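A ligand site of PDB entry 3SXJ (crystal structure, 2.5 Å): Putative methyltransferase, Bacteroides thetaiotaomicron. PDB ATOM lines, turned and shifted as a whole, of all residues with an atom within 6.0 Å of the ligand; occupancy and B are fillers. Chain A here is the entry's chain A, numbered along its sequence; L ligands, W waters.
The side-chain carboxylate of Asp 82 lies within hydrogen-bond range of an oxygen (O4) of the ligand, at 2.5 Å.
The backbone carbonyl oxygen (O) of Gly 60 is in hydrogen-bond range of a nitrogen (N1) of the ligand (2.8 Å).
N1 of the ligand lies within hydrogen-bond range of O of Glu 127, at 2.8 Å.
N of Met 111 lies within hydrogen-bond range of N5 of the ligand (2.8 Å).
OE1 of Gln 66 lies close to O2 of the ligand, at 3.0 Å.
The side-chain amide oxygen of Asn 132 lies close to an oxygen (O3) of the ligand, at 3.4 Å.
The guanidinium group (NE) of Arg 31 is in salt-bridge range of an oxygen (O2) of the ligand, at 3.0 Å.
N of Gln 32 lies within hydrogen-bond range of O2 of the ligand (3.2 Å).
N of Gly 62 lies close to O4 of the ligand, 3.5 Å away.
N6 of the ligand is in hydrogen-bond range of N of Leu 83 (3.4 Å).
The side-chain carboxylate of Asp 82 lies within hydrogen-bond range of the backbone NH of Phe 84 (3.4 Å).
O of Ile 81 lies within hydrogen-bond range of N of Gly 60.
NH2 of Arg 31 lies within salt-bridge range of OE2 of Glu 127 (3.0 Å).
The side-chain amide oxygen (OE1) of Gln 66 is in hydrogen-bond range of the guanidinium group (NE) of Arg 31 (3.3 Å).
The side-chain amide nitrogen (NE2) of Gln 66 is in hydrogen-bond range of the backbone carbonyl oxygen (O) of Cys 61 (3.2 Å).
The side-chain amide nitrogen of Asn 132 lies close to the side-chain hydroxyl of Tyr 131 (3.5 Å).
The backbone NH (N) of Cys 61 lies within hydrogen-bond range of the backbone carbonyl oxygen (O) of Ile 81 (3.2 Å).
OG of Ser 110 lies within hydrogen-bond range of OD1 of Asp 112, 2.9 Å away.
A sulfur (S1) of the ligand lies close to the backbone carbonyl oxygen (O) of Gly 128, at 3.7 Å.
Residues that only touch the ligand: Gly 33 (3.7 Å), Cys 61 (3.2 Å), Phe 84 (3.2 Å), Phe 87 (3.7 Å), Gly 109 (3.8 Å), Ser 110 (3.5 Å), Ala 129 (3.8 Å) and Tyr 131 (3.97 Å).
Hydrophobic or aromatic side chains that line the ligand: Leu 83, Phe 84, Phe 87, Met 111 and Ala 129.
Within 4 Å of the ligand: Arg 31, Gln 32, Gly 33, Gly 60, Cys 61, Gly 62, Gln 66, Asp 82, Leu 83, Phe 84, Phe 87, Gly 109, Ser 110, Met 111, Glu 127, Gly 128, Ala 129, Tyr 131 and Asn 132.
Along chain A the residues within 4 Å of the ligand span positions 31 to 132.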
ATOM      1  N   LYS A  30      14.693   3.290  15.467  1.00  0.00           N
ATOM      2  CA  LYS A  30      14.476   4.289  16.505  1.00  0.00           C
ATOM      3  C   LYS A  30      12.994   4.479  16.774  1.00  0.00           C
ATOM      4  O   LYS A  30      12.611   5.077  17.782  1.00  0.00           O
ATOM      5  CB  LYS A  30      15.129   5.616  16.119  1.00  0.00           C
ATOM      6  CG  LYS A  30      14.703   6.798  16.977  1.00  0.00           C
ATOM      7  CD  LYS A  30      15.333   8.098  16.506  1.00  0.00           C
ATOM      8  CE  LYS A  30      14.651   9.319  17.141  1.00  0.00           C
ATOM      9  NZ  LYS A  30      14.523   9.255  18.637  1.00  0.00           N
ATOM     10  N   ARG A  31      12.168   3.989  15.849  1.00  0.00           N
ATOM     11  CA  ARG A  31      10.709   4.058  15.971  1.00  0.00           C
ATOM     12  C   ARG A  31      10.158   2.771  15.359  1.00  0.00           C
ATOM     13  O   ARG A  31      10.594   2.346  14.284  1.00  0.00           O
ATOM     14  CB  ARG A  31      10.111   5.266  15.206  1.00  0.00           C
ATOM     15  CG  ARG A  31      10.386   6.641  15.804  1.00  0.00           C
ATOM     16  CD  ARG A  31       9.828   6.789  17.212  1.00  0.00           C
ATOM     17  NE  ARG A  31       8.385   6.609  17.268  1.00  0.00           N
ATOM     18  CZ  ARG A  31       7.475   7.548  17.016  1.00  0.00           C
ATOM     19  NH1 ARG A  31       7.847   8.780  16.693  1.00  0.00           N
ATOM     20  NH2 ARG A  31       6.185   7.264  17.095  1.00  0.00           N
ATOM     21  N   GLN A  32       9.199   2.143  16.055  1.00  0.00           N
ATOM     22  CA  GLN A  32       8.626   0.906  15.545  1.00  0.00           C
ATOM     23  C   GLN A  32       7.262   1.171  14.906  1.00  0.00           C
ATOM     24  O   GLN A  32       6.582   0.260  14.466  1.00  0.00           O
ATOM     25  CB  GLN A  32       8.492  -0.128  16.662  1.00  0.00           C
ATOM     26  CG  GLN A  32       9.807  -0.572  17.283  1.00  0.00           C
ATOM     27  CD  GLN A  32      10.471   0.509  18.129  1.00  0.00           C
ATOM     28  OE1 GLN A  32       9.854   1.056  19.051  1.00  0.00           O
ATOM     29  NE2 GLN A  32      11.735   0.820  17.820  1.00  0.00           N
ATOM     30  N   GLY A  33       6.897   2.450  14.865  1.00  0.00           N
ATOM     31  CA  GLY A  33       5.625   2.874  14.284  1.00  0.00           C
ATOM     32  C   GLY A  33       5.747   4.277  13.714  1.00  0.00           C
ATOM     33  O   GLY A  33       6.691   4.980  14.063  1.00  0.00           O
ATOM     34  N   PRO A  34       4.821   4.716  12.838  1.00  0.00           N
ATOM     35  CA  PRO A  34       4.851   6.059  12.225  1.00  0.00           C
ATOM     36  C   PRO A  34       4.696   7.200  13.228  1.00  0.00           C
ATOM     37  O   PRO A  34       3.895   7.114  14.150  1.00  0.00           O
ATOM     38  CB  PRO A  34       3.688   6.027  11.235  1.00  0.00           C
ATOM     39  CG  PRO A  34       3.494   4.558  10.953  1.00  0.00           C
ATOM     40  CD  PRO A  34       3.686   3.942  12.307  1.00  0.00           C
ATOM     41  N   ASP A  58       3.228   6.086  29.004  1.00  0.00           N
ATOM     42  CA  ASP A  58       3.257   5.842  27.568  1.00  0.00           C
ATOM     43  C   ASP A  58       3.065   4.331  27.346  1.00  0.00           C
ATOM     44  O   ASP A  58       3.997   3.560  27.501  1.00  0.00           O
ATOM     45  CB  ASP A  58       4.593   6.301  26.989  1.00  0.00           C
ATOM     46  CG  ASP A  58       4.627   6.209  25.478  1.00  0.00           C
ATOM     47  OD1 ASP A  58       3.588   5.825  24.889  1.00  0.00           O
ATOM     48  OD2 ASP A  58       5.681   6.525  24.895  1.00  0.00           O
ATOM     49  N   ILE A  59       1.847   3.939  26.982  1.00  0.00           N
ATOM     50  CA  ILE A  59       1.515   2.543  26.751  1.00  0.00           C
ATOM     51  C   ILE A  59       1.880   2.022  25.367  1.00  0.00           C
ATOM     52  O   ILE A  59       1.454   2.557  24.348  1.00  0.00           O
ATOM     53  CB  ILE A  59       0.006   2.307  26.992  1.00  0.00           C
ATOM     54  CG1 ILE A  59      -0.292   2.459  28.485  1.00  0.00           C
ATOM     55  CG2 ILE A  59      -0.425   0.930  26.485  1.00  0.00           C
ATOM     56  CD1 ILE A  59      -1.769   2.551  28.796  1.00  0.00           C
ATOM     57  N   GLY A  60       2.660   0.949  25.337  1.00  0.00           N
ATOM     58  CA  GLY A  60       3.103   0.376  24.074  1.00  0.00           C
ATOM     59  C   GLY A  60       4.228   1.256  23.568  1.00  0.00           C
ATOM     60  O   GLY A  60       4.357   1.515  22.371  1.00  0.00           O
ATOM     61  N   CYS A  61       5.066   1.690  24.505  1.00  0.00           N
ATOM     62  CA  CYS A  61       6.169   2.590  24.223  1.00  0.00           C
ATOM     63  C   CYS A  61       7.225   2.105  23.242  1.00  0.00           C
ATOM     64  O   CYS A  61       7.768   2.904  22.498  1.00  0.00           O
ATOM     65  CB  CYS A  61       6.853   2.999  25.530  1.00  0.00           C
ATOM     66  SG  CYS A  61       7.890   1.705  26.260  1.00  0.00           S
ATOM     67  N   GLY A  62       7.493   0.804  23.201  1.00  0.00           N
ATOM     68  CA  GLY A  62       8.512   0.321  22.289  1.00  0.00           C
ATOM     69  C   GLY A  62       9.900   0.713  22.783  1.00  0.00           C
ATOM     70  O   GLY A  62      10.173   0.667  23.980  1.00  0.00           O
ATOM     71  N   THR A  63      10.787   1.116  21.887  1.00  0.00           N
ATOM     72  CA  THR A  63      12.120   1.515  22.299  1.00  0.00           C
ATOM     73  C   THR A  63      12.084   2.848  23.032  1.00  0.00           C
ATOM     74  O   THR A  63      13.042   3.233  23.702  1.00  0.00           O
ATOM     75  CB  THR A  63      13.037   1.659  21.103  1.00  0.00           C
ATOM     76  OG1 THR A  63      12.367   2.415  20.097  1.00  0.00           O
ATOM     77  CG2 THR A  63      13.401   0.305  20.552  1.00  0.00           C
ATOM     78  N   GLY A  64      10.968   3.548  22.886  1.00  0.00           N
ATOM     79  CA  GLY A  64      10.825   4.831  23.539  1.00  0.00           C
ATOM     80  C   GLY A  64      11.184   5.985  22.631  1.00  0.00           C
ATOM     81  O   GLY A  64      11.568   7.060  23.100  1.00  0.00           O
ATOM     82  N   GLY A  65      11.065   5.770  21.327  1.00  0.00           N
ATOM     83  CA  GLY A  65      11.371   6.820  20.381  1.00  0.00           C
ATOM     84  C   GLY A  65      10.557   8.067  20.652  1.00  0.00           C
ATOM     85  O   GLY A  65      11.116   9.147  20.797  1.00  0.00           O
ATOM     86  N   GLN A  66       9.245   7.913  20.763  1.00  0.00           N
ATOM     87  CA  GLN A  66       8.389   9.060  21.004  1.00  0.00           C
ATOM     88  C   GLN A  66       8.275   9.432  22.462  1.00  0.00           C
ATOM     89  O   GLN A  66       7.819  10.529  22.792  1.00  0.00           O
ATOM     90  CB  GLN A  66       6.991   8.830  20.399  1.00  0.00           C
ATOM     91  CG  GLN A  66       6.135   7.824  21.127  1.00  0.00           C
ATOM     92  CD  GLN A  66       6.812   6.498  21.308  1.00  0.00           C
ATOM     93  OE1 GLN A  66       7.322   5.912  20.356  1.00  0.00           O
ATOM     94  NE2 GLN A  66       6.808   5.995  22.537  1.00  0.00           N
ATOM     95  N   ILE A  81       5.650   1.665  29.117  1.00  0.00           N
ATOM     96  CA  ILE A  81       5.334   0.265  29.335  1.00  0.00           C
ATOM     97  C   ILE A  81       5.218  -0.469  28.018  1.00  0.00           C
ATOM     98  O   ILE A  81       4.460  -0.065  27.146  1.00  0.00           O
ATOM     99  CB  ILE A  81       4.003   0.105  30.070  1.00  0.00           C
ATOM    100  CG1 ILE A  81       4.065   0.865  31.389  1.00  0.00           C
ATOM    101  CG2 ILE A  81       3.707  -1.361  30.294  1.00  0.00           C
ATOM    102  CD1 ILE A  81       2.909   0.551  32.329  1.00  0.00           C
ATOM    103  N   ASP A  82       5.959  -1.557  27.881  1.00  0.00           N
ATOM    104  CA  ASP A  82       5.905  -2.367  26.658  1.00  0.00           C
ATOM    105  C   ASP A  82       5.907  -3.852  27.055  1.00  0.00           C
ATOM    106  O   ASP A  82       6.271  -4.203  28.179  1.00  0.00           O
ATOM    107  CB  ASP A  82       7.089  -2.061  25.734  1.00  0.00           C
ATOM    108  CG  ASP A  82       6.837  -2.507  24.297  1.00  0.00           C
ATOM    109  OD1 ASP A  82       5.954  -1.921  23.654  1.00  0.00           O
ATOM    110  OD2 ASP A  82       7.515  -3.427  23.803  1.00  0.00           O
ATOM    111  N   LEU A  83       5.500  -4.697  26.121  1.00  0.00           N
ATOM    112  CA  LEU A  83       5.469  -6.126  26.378  1.00  0.00           C
ATOM    113  C   LEU A  83       6.872  -6.741  26.348  1.00  0.00           C
ATOM    114  O   LEU A  83       7.268  -7.482  27.254  1.00  0.00           O
ATOM    115  CB  LEU A  83       4.575  -6.808  25.349  1.00  0.00           C
ATOM    116  CG  LEU A  83       4.408  -8.316  25.491  1.00  0.00           C
ATOM    117  CD1 LEU A  83       3.744  -8.653  26.821  1.00  0.00           C
ATOM    118  CD2 LEU A  83       3.564  -8.820  24.331  1.00  0.00           C
ATOM    119  N   PHE A  84       7.623  -6.427  25.302  1.00  0.00           N
ATOM    120  CA  PHE A  84       8.970  -6.962  25.114  1.00  0.00           C
ATOM    121  C   PHE A  84      10.070  -6.339  25.967  1.00  0.00           C
ATOM    122  O   PHE A  84      10.327  -5.145  25.867  1.00  0.00           O
ATOM    123  CB  PHE A  84       9.384  -6.861  23.646  1.00  0.00           C
ATOM    124  CG  PHE A  84       8.563  -7.704  22.739  1.00  0.00           C
ATOM    125  CD1 PHE A  84       7.313  -7.271  22.321  1.00  0.00           C
ATOM    126  CD2 PHE A  84       9.007  -8.971  22.371  1.00  0.00           C
ATOM    127  CE1 PHE A  84       6.502  -8.089  21.534  1.00  0.00           C
ATOM    128  CE2 PHE A  84       8.205  -9.792  21.584  1.00  0.00           C
ATOM    129  CZ  PHE A  84       6.955  -9.359  21.166  1.00  0.00           C
ATOM    130  N   PHE A  87      12.972  -4.347  24.262  1.00  0.00           N
ATOM    131  CA  PHE A  87      12.713  -2.940  23.963  1.00  0.00           C
ATOM    132  C   PHE A  87      12.947  -2.093  25.214  1.00  0.00           C
ATOM    133  O   PHE A  87      13.708  -1.114  25.185  1.00  0.00           O
ATOM    134  CB  PHE A  87      11.272  -2.744  23.467  1.00  0.00           C
ATOM    135  CG  PHE A  87      11.028  -3.221  22.061  1.00  0.00           C
ATOM    136  CD1 PHE A  87      12.071  -3.293  21.150  1.00  0.00           C
ATOM    137  CD2 PHE A  87       9.739  -3.554  21.639  1.00  0.00           C
ATOM    138  CE1 PHE A  87      11.839  -3.687  19.831  1.00  0.00           C
ATOM    139  CE2 PHE A  87       9.507  -3.948  20.320  1.00  0.00           C
ATOM    140  CZ  PHE A  87      10.561  -4.016  19.416  1.00  0.00           C
ATOM    141  N   GLY A 109       5.572  -4.792  30.747  1.00  0.00           N
ATOM    142  CA  GLY A 109       4.212  -4.971  31.226  1.00  0.00           C
ATOM    143  C   GLY A 109       3.288  -5.214  30.064  1.00  0.00           C
ATOM    144  O   GLY A 109       3.719  -5.207  28.916  1.00  0.00           O
ATOM    145  N   SER A 110       2.007  -5.422  30.358  1.00  0.00           N
ATOM    146  CA  SER A 110       1.038  -5.674  29.309  1.00  0.00           C
ATOM    147  C   SER A 110       0.042  -4.528  29.173  1.00  0.00           C
ATOM    148  O   SER A 110      -0.160  -3.736  30.071  1.00  0.00           O
ATOM    149  CB  SER A 110       0.295  -6.985  29.554  1.00  0.00           C
ATOM    150  OG  SER A 110      -0.353  -7.445  28.381  1.00  0.00           O
ATOM    151  N   MET A 111      -0.603  -4.478  28.020  1.00  0.00           N
ATOM    152  CA  MET A 111      -1.559  -3.446  27.682  1.00  0.00           C
ATOM    153  C   MET A 111      -2.960  -3.765  28.204  1.00  0.00           C
ATOM    154  O   MET A 111      -3.773  -2.874  28.409  1.00  0.00           O
ATOM    155  CB  MET A 111      -1.572  -3.305  26.159  1.00  0.00           C
ATOM    156  CG  MET A 111      -2.095  -2.013  25.626  1.00  0.00           C
ATOM    157  SD  MET A 111      -2.123  -2.137  23.823  1.00  0.00           S
ATOM    158  CE  MET A 111      -0.373  -2.027  23.470  1.00  0.00           C
ATOM    159  N   ASP A 112      -3.228  -5.054  28.438  1.00  0.00           N
ATOM    160  CA  ASP A 112      -4.545  -5.478  28.930  1.00  0.00           C
ATOM    161  C   ASP A 112      -4.513  -5.755  30.428  1.00  0.00           C
ATOM    162  O   ASP A 112      -5.399  -6.424  30.968  1.00  0.00           O
ATOM    163  CB  ASP A 112      -5.009  -6.729  28.178  1.00  0.00           C
ATOM    164  CG  ASP A 112      -3.879  -7.724  27.948  1.00  0.00           C
ATOM    165  OD1 ASP A 112      -3.132  -8.014  28.911  1.00  0.00           O
ATOM    166  OD2 ASP A 112      -3.743  -8.235  26.814  1.00  0.00           O
ATOM    167  N   SER A 126       0.107   6.997  23.844  1.00  0.00           N
ATOM    168  CA  SER A 126       0.266   5.742  23.111  1.00  0.00           C
ATOM    169  C   SER A 126       0.259   5.934  21.592  1.00  0.00           C
ATOM    170  O   SER A 126      -0.761   6.315  20.999  1.00  0.00           O
ATOM    171  CB  SER A 126      -0.821   4.731  23.509  1.00  0.00           C
ATOM    172  OG  SER A 126      -0.648   3.475  22.848  1.00  0.00           O
ATOM    173  N   GLU A 127       1.398   5.649  20.971  1.00  0.00           N
ATOM    174  CA  GLU A 127       1.507   5.828  19.537  1.00  0.00           C
ATOM    175  C   GLU A 127       1.597   4.520  18.777  1.00  0.00           C
ATOM    176  O   GLU A 127       2.425   3.665  19.081  1.00  0.00           O
ATOM    177  CB  GLU A 127       2.718   6.726  19.226  1.00  0.00           C
ATOM    178  CG  GLU A 127       2.629   8.082  19.919  1.00  0.00           C
ATOM    179  CD  GLU A 127       3.461   9.152  19.248  1.00  0.00           C
ATOM    180  OE1 GLU A 127       3.653  10.227  19.863  1.00  0.00           O
ATOM    181  OE2 GLU A 127       3.894   8.920  18.117  1.00  0.00           O
ATOM    182  N   GLY A 128       0.711   4.370  17.788  1.00  0.00           N
ATOM    183  CA  GLY A 128       0.692   3.165  16.979  1.00  0.00           C
ATOM    184  C   GLY A 128       0.750   1.876  17.777  1.00  0.00           C
ATOM    185  O   GLY A 128       1.469   0.948  17.400  1.00  0.00           O
ATOM    186  N   ALA A 129      -0.002   1.820  18.877  1.00  0.00           N
ATOM    187  CA  ALA A 129      -0.032   0.624  19.720  1.00  0.00           C
ATOM    188  C   ALA A 129      -1.424   0.224  20.192  1.00  0.00           C
ATOM    189  O   ALA A 129      -1.665  -0.934  20.518  1.00  0.00           O
ATOM    190  CB  ALA A 129       0.898   0.801  20.936  1.00  0.00           C
ATOM    191  N   TYR A 131      -3.934  -0.426  18.684  1.00  0.00           N
ATOM    192  CA  TYR A 131      -4.469  -1.478  17.814  1.00  0.00           C
ATOM    193  C   TYR A 131      -4.348  -2.882  18.404  1.00  0.00           C
ATOM    194  O   TYR A 131      -5.129  -3.784  18.072  1.00  0.00           O
ATOM    195  CB  TYR A 131      -3.771  -1.425  16.449  1.00  0.00           C
ATOM    196  CG  TYR A 131      -2.363  -1.988  16.438  1.00  0.00           C
ATOM    197  CD1 TYR A 131      -2.135  -3.351  16.235  1.00  0.00           C
ATOM    198  CD2 TYR A 131      -1.255  -1.155  16.615  1.00  0.00           C
ATOM    199  CE1 TYR A 131      -0.847  -3.865  16.221  1.00  0.00           C
ATOM    200  CE2 TYR A 131       0.045  -1.666  16.594  1.00  0.00           C
ATOM    201  CZ  TYR A 131       0.242  -3.026  16.397  1.00  0.00           C
ATOM    202  OH  TYR A 131       1.520  -3.545  16.361  1.00  0.00           O
ATOM    203  N   ASN A 132      -3.356  -3.067  19.273  1.00  0.00           N
ATOM    204  CA  ASN A 132      -3.136  -4.354  19.902  1.00  0.00           C
ATOM    205  C   ASN A 132      -4.288  -4.822  20.797  1.00  0.00           C
ATOM    206  O   ASN A 132      -4.519  -6.023  20.941  1.00  0.00           O
ATOM    207  CB  ASN A 132      -1.822  -4.302  20.679  1.00  0.00           C
ATOM    208  CG  ASN A 132      -0.606  -4.269  19.770  1.00  0.00           C
ATOM    209  OD1 ASN A 132       0.391  -3.610  20.060  1.00  0.00           O
ATOM    210  ND2 ASN A 132      -0.688  -4.982  18.659  1.00  0.00           N
ATOM    211  N   ILE A 133      -5.030  -3.882  21.392  1.00  0.00           N
ATOM    212  CA  ILE A 133      -6.166  -4.253  22.238  1.00  0.00           C
ATOM    213  C   ILE A 133      -7.473  -3.622  21.789  1.00  0.00           C
ATOM    214  O   ILE A 133      -8.460  -3.677  22.506  1.00  0.00           O
ATOM    215  CB  ILE A 133      -6.003  -3.843  23.694  1.00  0.00           C
ATOM    216  CG1 ILE A 133      -5.822  -2.335  23.773  1.00  0.00           C
ATOM    217  CG2 ILE A 133      -4.836  -4.566  24.313  1.00  0.00           C
ATOM    218  CD1 ILE A 133      -5.897  -1.831  25.167  1.00  0.00           C
ATOM    219  N   TYR A 255      -2.255   7.377   9.931  1.00  0.00           N
ATOM    220  CA  TYR A 255      -2.346   7.470  11.367  1.00  0.00           C
ATOM    221  C   TYR A 255      -3.006   8.790  11.755  1.00  0.00           C
ATOM    222  O   TYR A 255      -2.750   9.830  11.134  1.00  0.00           O
ATOM    223  CB  TYR A 255      -0.940   7.383  11.982  1.00  0.00           C
ATOM    224  CG  TYR A 255      -0.528   5.999  12.451  1.00  0.00           C
ATOM    225  CD1 TYR A 255      -0.939   4.833  11.788  1.00  0.00           C
ATOM    226  CD2 TYR A 255       0.287   5.851  13.570  1.00  0.00           C
ATOM    227  CE1 TYR A 255      -0.548   3.568  12.240  1.00  0.00           C
ATOM    228  CE2 TYR A 255       0.680   4.594  14.029  1.00  0.00           C
ATOM    229  CZ  TYR A 255       0.260   3.460  13.364  1.00  0.00           C
ATOM    230  OH  TYR A 255       0.656   2.208  13.801  1.00  0.00           O
HETATM  231  N1  LIG L   1       4.844   3.386  20.403  1.00  0.00           N
HETATM  232  C1  LIG L   1       6.131   2.984  19.805  1.00  0.00           C
HETATM  233  C2  LIG L   1       6.414   3.878  18.599  1.00  0.00           C
HETATM  234  O1  LIG L   1       5.458   4.545  18.159  1.00  0.00           O
HETATM  235  O2  LIG L   1       7.585   3.884  18.151  1.00  0.00           O
HETATM  236  C3  LIG L   1       6.059   1.524  19.359  1.00  0.00           C
HETATM  237  C4  LIG L   1       4.987   1.306  18.288  1.00  0.00           C
HETATM  238  S1  LIG L   1       4.857  -0.438  17.745  1.00  0.00           S
HETATM  239  C5  LIG L   1       3.829  -0.241  16.306  1.00  0.00           C
HETATM  240  C6  LIG L   1       3.726  -1.360  18.836  1.00  0.00           C
HETATM  241  C7  LIG L   1       4.282  -1.484  20.260  1.00  0.00           C
HETATM  242  O3  LIG L   1       3.276  -2.097  21.087  1.00  0.00           O
HETATM  243  C8  LIG L   1       5.503  -2.400  20.292  1.00  0.00           C
HETATM  244  O4  LIG L   1       6.483  -1.868  21.187  1.00  0.00           O
HETATM  245  C9  LIG L   1       4.920  -3.697  20.850  1.00  0.00           C
HETATM  246  O5  LIG L   1       5.927  -4.436  21.546  1.00  0.00           O
HETATM  247  C10 LIG L   1       3.965  -3.095  21.870  1.00  0.00           C
HETATM  248  N2  LIG L   1       2.985  -4.077  22.385  1.00  0.00           N
HETATM  249  C11 LIG L   1       2.417  -5.064  21.679  1.00  0.00           C
HETATM  250  N3  LIG L   1       1.584  -5.739  22.464  1.00  0.00           N
HETATM  251  C12 LIG L   1       1.613  -5.190  23.675  1.00  0.00           C
HETATM  252  C13 LIG L   1       0.965  -5.449  24.873  1.00  0.00           C
HETATM  253  N4  LIG L   1       0.103  -6.457  24.977  1.00  0.00           N
HETATM  254  N5  LIG L   1       1.224  -4.666  25.931  1.00  0.00           N
HETATM  255  C14 LIG L   1       2.089  -3.674  25.843  1.00  0.00           C
HETATM  256  N6  LIG L   1       2.726  -3.400  24.722  1.00  0.00           N
HETATM  257  C15 LIG L   1       2.509  -4.132  23.627  1.00  0.00           C
HETATM  258  O   HOH W   1       4.273  -1.697  13.495  1.00  0.00           O
HETATM  259  O   HOH W   2       3.142   4.595  22.646  1.00  0.00           O
